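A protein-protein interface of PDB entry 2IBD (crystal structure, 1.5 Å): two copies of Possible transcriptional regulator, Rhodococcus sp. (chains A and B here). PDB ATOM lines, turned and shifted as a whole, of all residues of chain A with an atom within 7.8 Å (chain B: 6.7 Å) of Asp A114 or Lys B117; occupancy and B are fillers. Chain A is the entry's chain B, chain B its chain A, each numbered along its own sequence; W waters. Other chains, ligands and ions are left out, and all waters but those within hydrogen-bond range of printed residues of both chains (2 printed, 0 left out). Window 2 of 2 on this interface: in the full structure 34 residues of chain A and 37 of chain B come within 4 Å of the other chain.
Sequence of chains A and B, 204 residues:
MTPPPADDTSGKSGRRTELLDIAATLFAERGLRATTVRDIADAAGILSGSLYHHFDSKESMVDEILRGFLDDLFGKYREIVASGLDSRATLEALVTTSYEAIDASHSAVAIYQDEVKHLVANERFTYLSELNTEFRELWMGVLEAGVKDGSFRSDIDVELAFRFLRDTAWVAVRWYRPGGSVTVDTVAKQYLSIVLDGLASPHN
The guanidinium group (NH1) of Arg B174 is in hydrogen-bond range of the backbone carbonyl oxygen (O) of Gln A113 (2.9 Å).
The side-chain carboxylate of Asp A114 is in salt-bridge range of the side-chain amino group of Lys B117 (2.8 Å).
The side-chain carboxylate of Asp B114 lies within salt-bridge range of the guanidinium group of Arg A174 (3.0 Å).
The backbone carbonyl oxygen of Gln B113 sits at hydrogen-bond distance from the guanidinium group of Arg A174, 2.8 Å away.
NH2 of Arg B174 is in salt-bridge range of OD1 of Asp A114 (3.1 Å).
NE of Arg A174 lies close to NZ of Lys B117.
The side-chain carboxylate (OD2) of Asp B114 lies within salt-bridge range of the guanidinium group (NE) of Arg B174 (3.0 Å).
The guanidinium group (NE) of Arg A174 lies within salt-bridge range of the side-chain carboxylate (OD2) of Asp A114 (2.9 Å).
Of chain B, only Lys B117 (2.8 Å) and Arg B174 (3.1 Å) come within 4 Å of Asp A114.
Lys B117 touches just these residues of chain A: Asp A114 and Arg A174.
Of the printed residues of chain A, Asp B114 touches Arg A174 (3.0 Å).
Printed residues of chain A within 4 Å of Arg B174: Gln A113 (2.9 Å) and Asp A114 (3.1 Å).
Of the printed residues of chain B, Gln A113 touches Arg B174.
Leu A32 touches none of the printed residues of chain B.
Lys A117 touches none of the printed residues of chain B.
The nearest residue of chain B that does not touch Asp A114 is Asp B114 (4.1 Å).
The nearest residue of chain A that does not touch Lys B117 is Glu A115 (4.2 Å).
The nearest printed residue of chain A that does not touch Asp B114 is Asp A114 (4.1 Å).
Along chain B the printed residues that touch a printed residue of chain A span positions 113 to 174.
Among the printed residues, 6 pairs touch across the chains.
Gln A113 touches Arg B174, and with the chains exchanged Arg A174 touches Gln B113.
Asp A114 touches Lys B117, but with the chains exchanged Lys A117 does not touch Asp B114 (6.1 Å).
Asp A114 touches Arg B174, and with the chains exchanged Arg A174 touches Asp B114.
Arg A174 touches Lys B117, but with the chains exchanged Lys A117 does not touch Arg B174 (6.9 Å).
9 positions are printed for both chains.
Water W1 lies within hydrogen-bond range of OD2 of Asp A114 (2.7 Å) and NZ of Lys B117 (3.0 Å).
Water W2 lies within hydrogen-bond range of O of Asp A114 and O of Asp B114.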
ATOM      1  N   PHE A  27     -19.525  19.295 -12.862  1.00  0.00           N
ATOM      2  CA  PHE A  27     -18.711  18.916 -11.713  1.00  0.00           C
ATOM      3  C   PHE A  27     -18.812  17.420 -11.453  1.00  0.00           C
ATOM      4  O   PHE A  27     -17.813  16.754 -11.201  1.00  0.00           O
ATOM      5  CB  PHE A  27     -19.139  19.668 -10.459  1.00  0.00           C
ATOM      6  CG  PHE A  27     -18.958  21.153 -10.546  1.00  0.00           C
ATOM      7  CD1 PHE A  27     -17.965  21.706 -11.365  1.00  0.00           C
ATOM      8  CD2 PHE A  27     -19.723  22.010  -9.755  1.00  0.00           C
ATOM      9  CE1 PHE A  27     -17.785  23.105 -11.441  1.00  0.00           C
ATOM     10  CE2 PHE A  27     -19.533  23.411  -9.806  1.00  0.00           C
ATOM     11  CZ  PHE A  27     -18.569  23.955 -10.668  1.00  0.00           C
ATOM     12  N   ALA A  28     -20.030  16.893 -11.509  1.00  0.00           N
ATOM     13  CA  ALA A  28     -20.236  15.471 -11.232  1.00  0.00           C
ATOM     14  C   ALA A  28     -19.665  14.594 -12.348  1.00  0.00           C
ATOM     15  O   ALA A  28     -19.183  13.494 -12.078  1.00  0.00           O
ATOM     16  CB  ALA A  28     -21.722  15.186 -11.036  1.00  0.00           C
ATOM     17  N   GLU A  29     -19.740  15.076 -13.595  1.00  0.00           N
ATOM     18  CA  GLU A  29     -19.360  14.264 -14.760  1.00  0.00           C
ATOM     19  C   GLU A  29     -17.874  14.355 -15.130  1.00  0.00           C
ATOM     20  O   GLU A  29     -17.261  13.334 -15.439  1.00  0.00           O
ATOM     21  CB  GLU A  29     -20.282  14.563 -15.960  1.00  0.00           C
ATOM     22  CG  GLU A  29     -21.726  14.062 -15.737  1.00  0.00           C
ATOM     23  CD  GLU A  29     -22.665  14.234 -16.942  1.00  0.00           C
ATOM     24  OE1 GLU A  29     -22.279  14.862 -17.947  1.00  0.00           O
ATOM     25  OE2 GLU A  29     -23.804  13.725 -16.870  1.00  0.00           O
ATOM     26  N   GLY A  31     -15.605  16.246 -12.938  1.00  0.00           N
ATOM     27  CA  GLY A  31     -14.871  16.542 -11.707  1.00  0.00           C
ATOM     28  C   GLY A  31     -14.610  18.036 -11.617  1.00  0.00           C
ATOM     29  O   GLY A  31     -14.554  18.729 -12.647  1.00  0.00           O
ATOM     30  N   LEU A  32     -14.414  18.517 -10.391  1.00  0.00           N
ATOM     31  CA  LEU A  32     -14.253  19.936 -10.087  1.00  0.00           C
ATOM     32  C   LEU A  32     -13.050  20.542 -10.769  1.00  0.00           C
ATOM     33  O   LEU A  32     -13.174  21.581 -11.395  1.00  0.00           O
ATOM     34  CB  LEU A  32     -14.125  20.170  -8.581  1.00  0.00           C
ATOM     35  CG  LEU A  32     -15.408  20.420  -7.792  1.00  0.00           C
ATOM     36  CD1 LEU A  32     -16.385  19.240  -7.846  1.00  0.00           C
ATOM     37  CD2 LEU A  32     -15.056  20.782  -6.365  1.00  0.00           C
ATOM     38  N   ARG A  33     -11.891  19.897 -10.646  1.00  0.00           N
ATOM     39  CA  ARG A  33     -10.636  20.489 -11.150  1.00  0.00           C
ATOM     40  C   ARG A  33     -10.476  20.436 -12.666  1.00  0.00           C
ATOM     41  O   ARG A  33      -9.706  21.211 -13.239  1.00  0.00           O
ATOM     42  CB  ARG A  33      -9.422  19.894 -10.436  1.00  0.00           C
ATOM     43  CG  ARG A  33      -9.323  20.398  -9.002  1.00  0.00           C
ATOM     44  CD  ARG A  33      -8.229  19.703  -8.236  1.00  0.00           C
ATOM     45  NE  ARG A  33      -8.604  18.325  -7.926  1.00  0.00           N
ATOM     46  CZ  ARG A  33      -7.840  17.485  -7.229  1.00  0.00           C
ATOM     47  NH1 ARG A  33      -6.656  17.877  -6.759  1.00  0.00           N
ATOM     48  NH2 ARG A  33      -8.264  16.253  -6.999  1.00  0.00           N
ATOM     49  N   SER A 107     -26.561  15.149  -8.889  1.00  0.00           N
ATOM     50  CA  SER A 107     -25.232  15.738  -9.087  1.00  0.00           C
ATOM     51  C   SER A 107     -24.581  16.172  -7.792  1.00  0.00           C
ATOM     52  O   SER A 107     -23.378  16.000  -7.617  1.00  0.00           O
ATOM     53  CB  SER A 107     -25.331  16.924 -10.043  1.00  0.00           C
ATOM     54  OG  SER A 107     -25.688  16.436 -11.311  1.00  0.00           O
ATOM     55  N   ALA A 108     -25.375  16.758  -6.900  1.00  0.00           N
ATOM     56  CA  ALA A 108     -24.844  17.226  -5.617  1.00  0.00           C
ATOM     57  C   ALA A 108     -24.323  16.050  -4.809  1.00  0.00           C
ATOM     58  O   ALA A 108     -23.285  16.170  -4.159  1.00  0.00           O
ATOM     59  CB  ALA A 108     -25.902  17.995  -4.838  1.00  0.00           C
ATOM     60  N   VAL A 109     -25.056  14.923  -4.836  1.00  0.00           N
ATOM     61  CA  VAL A 109     -24.621  13.761  -4.093  1.00  0.00           C
ATOM     62  C   VAL A 109     -23.325  13.250  -4.704  1.00  0.00           C
ATOM     63  O   VAL A 109     -22.423  12.918  -3.946  1.00  0.00           O
ATOM     64  CB  VAL A 109     -25.692  12.654  -4.042  1.00  0.00           C
ATOM     65  CG1 VAL A 109     -25.125  11.379  -3.331  1.00  0.00           C
ATOM     66  CG2 VAL A 109     -26.949  13.167  -3.301  1.00  0.00           C
ATOM     67  N   ALA A 110     -23.233  13.197  -6.040  1.00  0.00           N
ATOM     68  CA  ALA A 110     -22.008  12.713  -6.674  1.00  0.00           C
ATOM     69  C   ALA A 110     -20.827  13.591  -6.303  1.00  0.00           C
ATOM     70  O   ALA A 110     -19.745  13.087  -6.028  1.00  0.00           O
ATOM     71  CB  ALA A 110     -22.162  12.626  -8.208  1.00  0.00           C
ATOM     72  N   ILE A 111     -21.027  14.909  -6.292  1.00  0.00           N
ATOM     73  CA  ILE A 111     -19.951  15.830  -5.908  1.00  0.00           C
ATOM     74  C   ILE A 111     -19.525  15.552  -4.452  1.00  0.00           C
ATOM     75  O   ILE A 111     -18.336  15.342  -4.179  1.00  0.00           O
ATOM     76  CB  ILE A 111     -20.379  17.304  -6.120  1.00  0.00           C
ATOM     77  CG1 ILE A 111     -20.649  17.567  -7.597  1.00  0.00           C
ATOM     78  CG2 ILE A 111     -19.337  18.306  -5.534  1.00  0.00           C
ATOM     79  CD1 ILE A 111     -21.511  18.793  -7.802  1.00  0.00           C
ATOM     80  N   TYR A 112     -20.501  15.489  -3.547  1.00  0.00           N
ATOM     81  CA  TYR A 112     -20.228  15.164  -2.139  1.00  0.00           C
ATOM     82  C   TYR A 112     -19.508  13.800  -1.928  1.00  0.00           C
ATOM     83  O   TYR A 112     -18.529  13.713  -1.169  1.00  0.00           O
ATOM     84  CB  TYR A 112     -21.545  15.169  -1.375  1.00  0.00           C
ATOM     85  CG  TYR A 112     -21.448  14.929   0.117  1.00  0.00           C
ATOM     86  CD1 TYR A 112     -20.801  15.828   0.954  1.00  0.00           C
ATOM     87  CD2 TYR A 112     -22.062  13.812   0.696  1.00  0.00           C
ATOM     88  CE1 TYR A 112     -20.737  15.604   2.335  1.00  0.00           C
ATOM     89  CE2 TYR A 112     -22.030  13.598   2.065  1.00  0.00           C
ATOM     90  CZ  TYR A 112     -21.356  14.482   2.870  1.00  0.00           C
ATOM     91  OH  TYR A 112     -21.322  14.250   4.234  1.00  0.00           O
ATOM     92  N   GLN A 113     -19.985  12.756  -2.604  1.00  0.00           N
ATOM     93  CA  GLN A 113     -19.478  11.382  -2.416  1.00  0.00           C
ATOM     94  C   GLN A 113     -18.122  11.162  -3.081  1.00  0.00           C
ATOM     95  O   GLN A 113     -17.262  10.469  -2.527  1.00  0.00           O
ATOM     96  CB  GLN A 113     -20.510  10.347  -2.902  1.00  0.00           C
ATOM     97  CG  GLN A 113     -20.040   8.874  -2.997  1.00  0.00           C
ATOM     98  CD  GLN A 113     -19.724   8.257  -1.635  1.00  0.00           C
ATOM     99  OE1 GLN A 113     -20.080   8.800  -0.592  1.00  0.00           O
ATOM    100  NE2 GLN A 113     -19.036   7.108  -1.651  1.00  0.00           N
ATOM    101  N   ASP A 114     -17.912  11.761  -4.250  1.00  0.00           N
ATOM    102  CA  ASP A 114     -16.762  11.364  -5.081  1.00  0.00           C
ATOM    103  C   ASP A 114     -15.793  12.475  -5.448  1.00  0.00           C
ATOM    104  O   ASP A 114     -14.686  12.176  -5.886  1.00  0.00           O
ATOM    105  CB  ASP A 114     -17.244  10.682  -6.369  1.00  0.00           C
ATOM    106  CG  ASP A 114     -17.663   9.238  -6.144  1.00  0.00           C
ATOM    107  OD1 ASP A 114     -17.099   8.578  -5.229  1.00  0.00           O
ATOM    108  OD2 ASP A 114     -18.537   8.744  -6.897  1.00  0.00           O
ATOM    109  N   GLU A 115     -16.206  13.734  -5.305  1.00  0.00           N
ATOM    110  CA  GLU A 115     -15.491  14.848  -5.947  1.00  0.00           C
ATOM    111  C   GLU A 115     -14.865  15.883  -5.017  1.00  0.00           C
ATOM    112  O   GLU A 115     -14.240  16.837  -5.495  1.00  0.00           O
ATOM    113  CB  GLU A 115     -16.391  15.565  -6.957  1.00  0.00           C
ATOM    114  CG  GLU A 115     -16.983  14.641  -8.015  1.00  0.00           C
ATOM    115  CD  GLU A 115     -15.946  13.971  -8.896  1.00  0.00           C
ATOM    116  OE1 GLU A 115     -14.869  14.577  -9.130  1.00  0.00           O
ATOM    117  OE2 GLU A 115     -16.215  12.843  -9.366  1.00  0.00           O
ATOM    118  N   VAL A 116     -14.979  15.708  -3.708  1.00  0.00           N
ATOM    119  CA  VAL A 116     -14.457  16.755  -2.827  1.00  0.00           C
ATOM    120  C   VAL A 116     -13.366  16.332  -1.826  1.00  0.00           C
ATOM    121  O   VAL A 116     -13.136  17.033  -0.830  1.00  0.00           O
ATOM    122  CB  VAL A 116     -15.594  17.543  -2.118  1.00  0.00           C
ATOM    123  CG1 VAL A 116     -16.468  18.275  -3.144  1.00  0.00           C
ATOM    124  CG2 VAL A 116     -16.435  16.643  -1.196  1.00  0.00           C
ATOM    125  N   LYS A 117     -12.687  15.207  -2.094  1.00  0.00           N
ATOM    126  CA  LYS A 117     -11.618  14.740  -1.188  1.00  0.00           C
ATOM    127  C   LYS A 117     -10.588  15.853  -0.971  1.00  0.00           C
ATOM    128  O   LYS A 117     -10.037  15.988   0.121  1.00  0.00           O
ATOM    129  CB  LYS A 117     -10.936  13.472  -1.730  1.00  0.00           C
ATOM    130  CG  LYS A 117      -9.957  12.773  -0.768  1.00  0.00           C
ATOM    131  CD  LYS A 117      -9.200  11.604  -1.448  1.00  0.00           C
ATOM    132  CE  LYS A 117      -8.270  10.914  -0.451  1.00  0.00           C
ATOM    133  NZ  LYS A 117      -7.475   9.748  -0.988  1.00  0.00           N
ATOM    134  N   HIS A 118     -10.360  16.657  -2.007  1.00  0.00           N
ATOM    135  CA  HIS A 118      -9.342  17.714  -1.967  1.00  0.00           C
ATOM    136  C   HIS A 118      -9.826  18.988  -1.263  1.00  0.00           C
ATOM    137  O   HIS A 118      -9.034  19.927  -1.046  1.00  0.00           O
ATOM    138  CB  HIS A 118      -8.859  18.045  -3.386  1.00  0.00           C
ATOM    139  CG  HIS A 118      -9.902  18.702  -4.230  1.00  0.00           C
ATOM    140  ND1 HIS A 118     -11.024  18.039  -4.677  1.00  0.00           N
ATOM    141  CD2 HIS A 118     -10.003  19.971  -4.691  1.00  0.00           C
ATOM    142  CE1 HIS A 118     -11.768  18.871  -5.386  1.00  0.00           C
ATOM    143  NE2 HIS A 118     -11.172  20.050  -5.408  1.00  0.00           N
ATOM    144  N   TRP A 170     -24.232   6.518   0.005  1.00  0.00           N
ATOM    145  CA  TRP A 170     -24.258   7.282  -1.246  1.00  0.00           C
ATOM    146  C   TRP A 170     -23.753   6.539  -2.467  1.00  0.00           C
ATOM    147  O   TRP A 170     -23.781   7.082  -3.569  1.00  0.00           O
ATOM    148  CB  TRP A 170     -23.437   8.559  -1.102  1.00  0.00           C
ATOM    149  CG  TRP A 170     -23.820   9.307   0.143  1.00  0.00           C
ATOM    150  CD1 TRP A 170     -23.040   9.501   1.265  1.00  0.00           C
ATOM    151  CD2 TRP A 170     -25.080   9.917   0.413  1.00  0.00           C
ATOM    152  NE1 TRP A 170     -23.756  10.212   2.208  1.00  0.00           N
ATOM    153  CE2 TRP A 170     -25.007  10.461   1.720  1.00  0.00           C
ATOM    154  CE3 TRP A 170     -26.273  10.052  -0.318  1.00  0.00           C
ATOM    155  CZ2 TRP A 170     -26.062  11.149   2.301  1.00  0.00           C
ATOM    156  CZ3 TRP A 170     -27.320  10.730   0.251  1.00  0.00           C
ATOM    157  CH2 TRP A 170     -27.211  11.282   1.556  1.00  0.00           C
ATOM    158  N   VAL A 171     -23.264   5.319  -2.269  1.00  0.00           N
ATOM    159  CA  VAL A 171     -22.580   4.596  -3.332  1.00  0.00           C
ATOM    160  C   VAL A 171     -23.439   4.342  -4.559  1.00  0.00           C
ATOM    161  O   VAL A 171     -22.886   4.325  -5.665  1.00  0.00           O
ATOM    162  CB  VAL A 171     -21.933   3.287  -2.835  1.00  0.00           C
ATOM    163  CG1 VAL A 171     -20.821   3.603  -1.835  1.00  0.00           C
ATOM    164  CG2 VAL A 171     -22.952   2.374  -2.203  1.00  0.00           C
ATOM    165  N   VAL A 173     -25.084   6.314  -6.076  1.00  0.00           N
ATOM    166  CA  VAL A 173     -25.046   7.482  -6.965  1.00  0.00           C
ATOM    167  C   VAL A 173     -24.300   7.232  -8.258  1.00  0.00           C
ATOM    168  O   VAL A 173     -24.571   7.872  -9.283  1.00  0.00           O
ATOM    169  CB  VAL A 173     -24.457   8.774  -6.271  1.00  0.00           C
ATOM    170  CG1 VAL A 173     -22.919   8.662  -6.097  1.00  0.00           C
ATOM    171  CG2 VAL A 173     -24.866  10.051  -7.051  1.00  0.00           C
ATOM    172  N   ARG A 174     -23.356   6.292  -8.243  1.00  0.00           N
ATOM    173  CA  ARG A 174     -22.604   6.079  -9.462  1.00  0.00           C
ATOM    174  C   ARG A 174     -23.441   5.493 -10.599  1.00  0.00           C
ATOM    175  O   ARG A 174     -23.121   5.702 -11.781  1.00  0.00           O
ATOM    176  CB  ARG A 174     -21.353   5.264  -9.214  1.00  0.00           C
ATOM    177  CG  ARG A 174     -20.311   6.059  -8.436  1.00  0.00           C
ATOM    178  CD  ARG A 174     -19.046   5.266  -8.317  1.00  0.00           C
ATOM    179  NE  ARG A 174     -18.065   5.967  -7.501  1.00  0.00           N
ATOM    180  CZ  ARG A 174     -16.858   5.467  -7.231  1.00  0.00           C
ATOM    181  NH1 ARG A 174     -16.513   4.277  -7.721  1.00  0.00           N
ATOM    182  NH2 ARG A 174     -16.000   6.157  -6.488  1.00  0.00           N
ATOM    183  N   ILE B 111      -6.973   3.164  -5.832  1.00  0.00           N
ATOM    184  CA  ILE B 111      -6.948   3.669  -7.195  1.00  0.00           C
ATOM    185  C   ILE B 111      -8.103   3.041  -7.991  1.00  0.00           C
ATOM    186  O   ILE B 111      -8.849   3.735  -8.688  1.00  0.00           O
ATOM    187  CB  ILE B 111      -5.590   3.306  -7.856  1.00  0.00           C
ATOM    188  CG1 ILE B 111      -4.459   4.066  -7.174  1.00  0.00           C
ATOM    189  CG2 ILE B 111      -5.618   3.560  -9.370  1.00  0.00           C
ATOM    190  CD1 ILE B 111      -3.077   3.391  -7.428  1.00  0.00           C
ATOM    191  N   TYR B 112      -8.290   1.730  -7.852  1.00  0.00           N
ATOM    192  CA  TYR B 112      -9.395   1.046  -8.535  1.00  0.00           C
ATOM    193  C   TYR B 112     -10.781   1.580  -8.160  1.00  0.00           C
ATOM    194  O   TYR B 112     -11.652   1.720  -9.012  1.00  0.00           O
ATOM    195  CB  TYR B 112      -9.307  -0.427  -8.200  1.00  0.00           C
ATOM    196  CG  TYR B 112     -10.167  -1.333  -9.040  1.00  0.00           C
ATOM    197  CD1 TYR B 112     -10.059  -1.331 -10.428  1.00  0.00           C
ATOM    198  CD2 TYR B 112     -11.051  -2.243  -8.440  1.00  0.00           C
ATOM    199  CE1 TYR B 112     -10.821  -2.192 -11.204  1.00  0.00           C
ATOM    200  CE2 TYR B 112     -11.818  -3.108  -9.211  1.00  0.00           C
ATOM    201  CZ  TYR B 112     -11.709  -3.064 -10.596  1.00  0.00           C
ATOM    202  OH  TYR B 112     -12.444  -3.939 -11.378  1.00  0.00           O
ATOM    203  N   GLN B 113     -10.974   1.863  -6.878  1.00  0.00           N
ATOM    204  CA  GLN B 113     -12.272   2.294  -6.368  1.00  0.00           C
ATOM    205  C   GLN B 113     -12.606   3.744  -6.708  1.00  0.00           C
ATOM    206  O   GLN B 113     -13.778   4.058  -7.011  1.00  0.00           O
ATOM    207  CB  GLN B 113     -12.332   2.089  -4.843  1.00  0.00           C
ATOM    208  CG  GLN B 113     -13.567   2.746  -4.146  1.00  0.00           C
ATOM    209  CD  GLN B 113     -14.912   2.187  -4.600  1.00  0.00           C
ATOM    210  OE1 GLN B 113     -14.999   1.150  -5.259  1.00  0.00           O
ATOM    211  NE2 GLN B 113     -15.983   2.909  -4.252  1.00  0.00           N
ATOM    212  N   ASP B 114     -11.620   4.639  -6.590  1.00  0.00           N
ATOM    213  CA  ASP B 114     -11.894   6.091  -6.572  1.00  0.00           C
ATOM    214  C   ASP B 114     -11.169   6.838  -7.638  1.00  0.00           C
ATOM    215  O   ASP B 114     -11.440   8.018  -7.824  1.00  0.00           O
ATOM    216  CB  ASP B 114     -11.543   6.744  -5.212  1.00  0.00           C
ATOM    217  CG  ASP B 114     -12.595   6.490  -4.158  1.00  0.00           C
ATOM    218  OD1 ASP B 114     -13.777   6.332  -4.519  1.00  0.00           O
ATOM    219  OD2 ASP B 114     -12.250   6.451  -2.952  1.00  0.00           O
ATOM    220  N   GLU B 115     -10.242   6.184  -8.342  1.00  0.00           N
ATOM    221  CA  GLU B 115      -9.325   6.933  -9.218  1.00  0.00           C
ATOM    222  C   GLU B 115      -9.350   6.682 -10.716  1.00  0.00           C
ATOM    223  O   GLU B 115      -8.628   7.390 -11.444  1.00  0.00           O
ATOM    224  CB  GLU B 115      -7.881   6.788  -8.743  1.00  0.00           C
ATOM    225  CG  GLU B 115      -7.441   7.896  -7.871  1.00  0.00           C
ATOM    226  CD  GLU B 115      -7.978   9.226  -8.369  1.00  0.00           C
ATOM    227  OE1 GLU B 115      -7.742   9.585  -9.558  1.00  0.00           O
ATOM    228  OE2 GLU B 115      -8.675   9.891  -7.565  1.00  0.00           O
ATOM    229  N   VAL B 116     -10.170   5.731 -11.164  1.00  0.00           N
ATOM    230  CA  VAL B 116     -10.129   5.233 -12.560  1.00  0.00           C
ATOM    231  C   VAL B 116     -11.367   5.477 -13.414  1.00  0.00           C
ATOM    232  O   VAL B 116     -11.503   4.904 -14.515  1.00  0.00           O
ATOM    233  CB  VAL B 116      -9.758   3.717 -12.633  1.00  0.00           C
ATOM    234  CG1 VAL B 116      -8.391   3.457 -11.967  1.00  0.00           C
ATOM    235  CG2 VAL B 116     -10.860   2.812 -12.044  1.00  0.00           C
ATOM    236  N   LYS B 117     -12.282   6.306 -12.911  1.00  0.00           N
ATOM    237  CA  LYS B 117     -13.464   6.692 -13.694  1.00  0.00           C
ATOM    238  C   LYS B 117     -13.067   7.149 -15.096  1.00  0.00           C
ATOM    239  O   LYS B 117     -13.664   6.756 -16.096  1.00  0.00           O
ATOM    240  CB  LYS B 117     -14.219   7.816 -12.981  1.00  0.00           C
ATOM    241  CG  LYS B 117     -15.059   7.301 -11.834  1.00  0.00           C
ATOM    242  CD  LYS B 117     -15.235   8.348 -10.756  1.00  0.00           C
ATOM    243  CE  LYS B 117     -16.111   7.796  -9.650  1.00  0.00           C
ATOM    244  NZ  LYS B 117     -17.152   8.787  -9.277  1.00  0.00           N
ATOM    245  N   HIS B 118     -12.019   7.949 -15.142  1.00  0.00           N
ATOM    246  CA  HIS B 118     -11.587   8.591 -16.363  1.00  0.00           C
ATOM    247  C   HIS B 118     -10.585   7.749 -17.187  1.00  0.00           C
ATOM    248  O   HIS B 118     -10.124   8.210 -18.236  1.00  0.00           O
ATOM    249  CB  HIS B 118     -10.946   9.926 -15.997  1.00  0.00           C
ATOM    250  CG  HIS B 118      -9.582   9.767 -15.407  1.00  0.00           C
ATOM    251  ND1 HIS B 118      -9.373   9.201 -14.168  1.00  0.00           N
ATOM    252  CD2 HIS B 118      -8.356  10.034 -15.915  1.00  0.00           C
ATOM    253  CE1 HIS B 118      -8.075   9.154 -13.924  1.00  0.00           C
ATOM    254  NE2 HIS B 118      -7.435   9.645 -14.972  1.00  0.00           N
ATOM    255  N   LEU B 119     -10.214   6.553 -16.724  1.00  0.00           N
ATOM    256  CA  LEU B 119      -9.344   5.697 -17.545  1.00  0.00           C
ATOM    257  C   LEU B 119     -10.113   4.971 -18.652  1.00  0.00           C
ATOM    258  O   LEU B 119      -9.505   4.449 -19.588  1.00  0.00           O
ATOM    259  CB  LEU B 119      -8.588   4.675 -16.701  1.00  0.00           C
ATOM    260  CG  LEU B 119      -7.527   5.223 -15.749  1.00  0.00           C
ATOM    261  CD1 LEU B 119      -6.972   4.085 -14.911  1.00  0.00           C
ATOM    262  CD2 LEU B 119      -6.416   5.953 -16.532  1.00  0.00           C
ATOM    263  N   VAL B 120     -11.439   4.946 -18.525  1.00  0.00           N
ATOM    264  CA  VAL B 120     -12.339   4.310 -19.504  1.00  0.00           C
ATOM    265  C   VAL B 120     -12.140   4.895 -20.898  1.00  0.00           C
ATOM    266  O   VAL B 120     -12.224   4.172 -21.890  1.00  0.00           O
ATOM    267  CB  VAL B 120     -13.829   4.448 -19.073  1.00  0.00           C
ATOM    268  CG1 VAL B 120     -14.776   3.818 -20.103  1.00  0.00           C
ATOM    269  CG2 VAL B 120     -14.037   3.814 -17.713  1.00  0.00           C
ATOM    270  N   ALA B 121     -11.850   6.193 -20.961  1.00  0.00           N
ATOM    271  CA  ALA B 121     -11.624   6.884 -22.226  1.00  0.00           C
ATOM    272  C   ALA B 121     -10.359   6.402 -22.967  1.00  0.00           C
ATOM    273  O   ALA B 121     -10.236   6.598 -24.179  1.00  0.00           O
ATOM    274  CB  ALA B 121     -11.556   8.401 -21.985  1.00  0.00           C
ATOM    275  N   ARG B 174     -11.454   3.529   2.161  1.00  0.00           N
ATOM    276  CA  ARG B 174     -11.357   4.942   2.567  1.00  0.00           C
ATOM    277  C   ARG B 174     -10.924   5.107   4.033  1.00  0.00           C
ATOM    278  O   ARG B 174     -10.332   6.134   4.368  1.00  0.00           O
ATOM    279  CB  ARG B 174     -12.682   5.681   2.274  1.00  0.00           C
ATOM    280  CG  ARG B 174     -12.937   5.881   0.759  1.00  0.00           C
ATOM    281  CD  ARG B 174     -14.121   6.853   0.469  1.00  0.00           C
ATOM    282  NE  ARG B 174     -14.343   7.095  -0.965  1.00  0.00           N
ATOM    283  CZ  ARG B 174     -15.210   7.989  -1.459  1.00  0.00           C
ATOM    284  NH1 ARG B 174     -15.926   8.771  -0.656  1.00  0.00           N
ATOM    285  NH2 ARG B 174     -15.341   8.138  -2.771  1.00  0.00           N
HETATM  286  O   HOH W   1     -19.972   9.848  -8.876  1.00  0.00           O
HETATM  287  O   HOH W   2     -13.748   9.359  -6.341  1.00  0.00           O
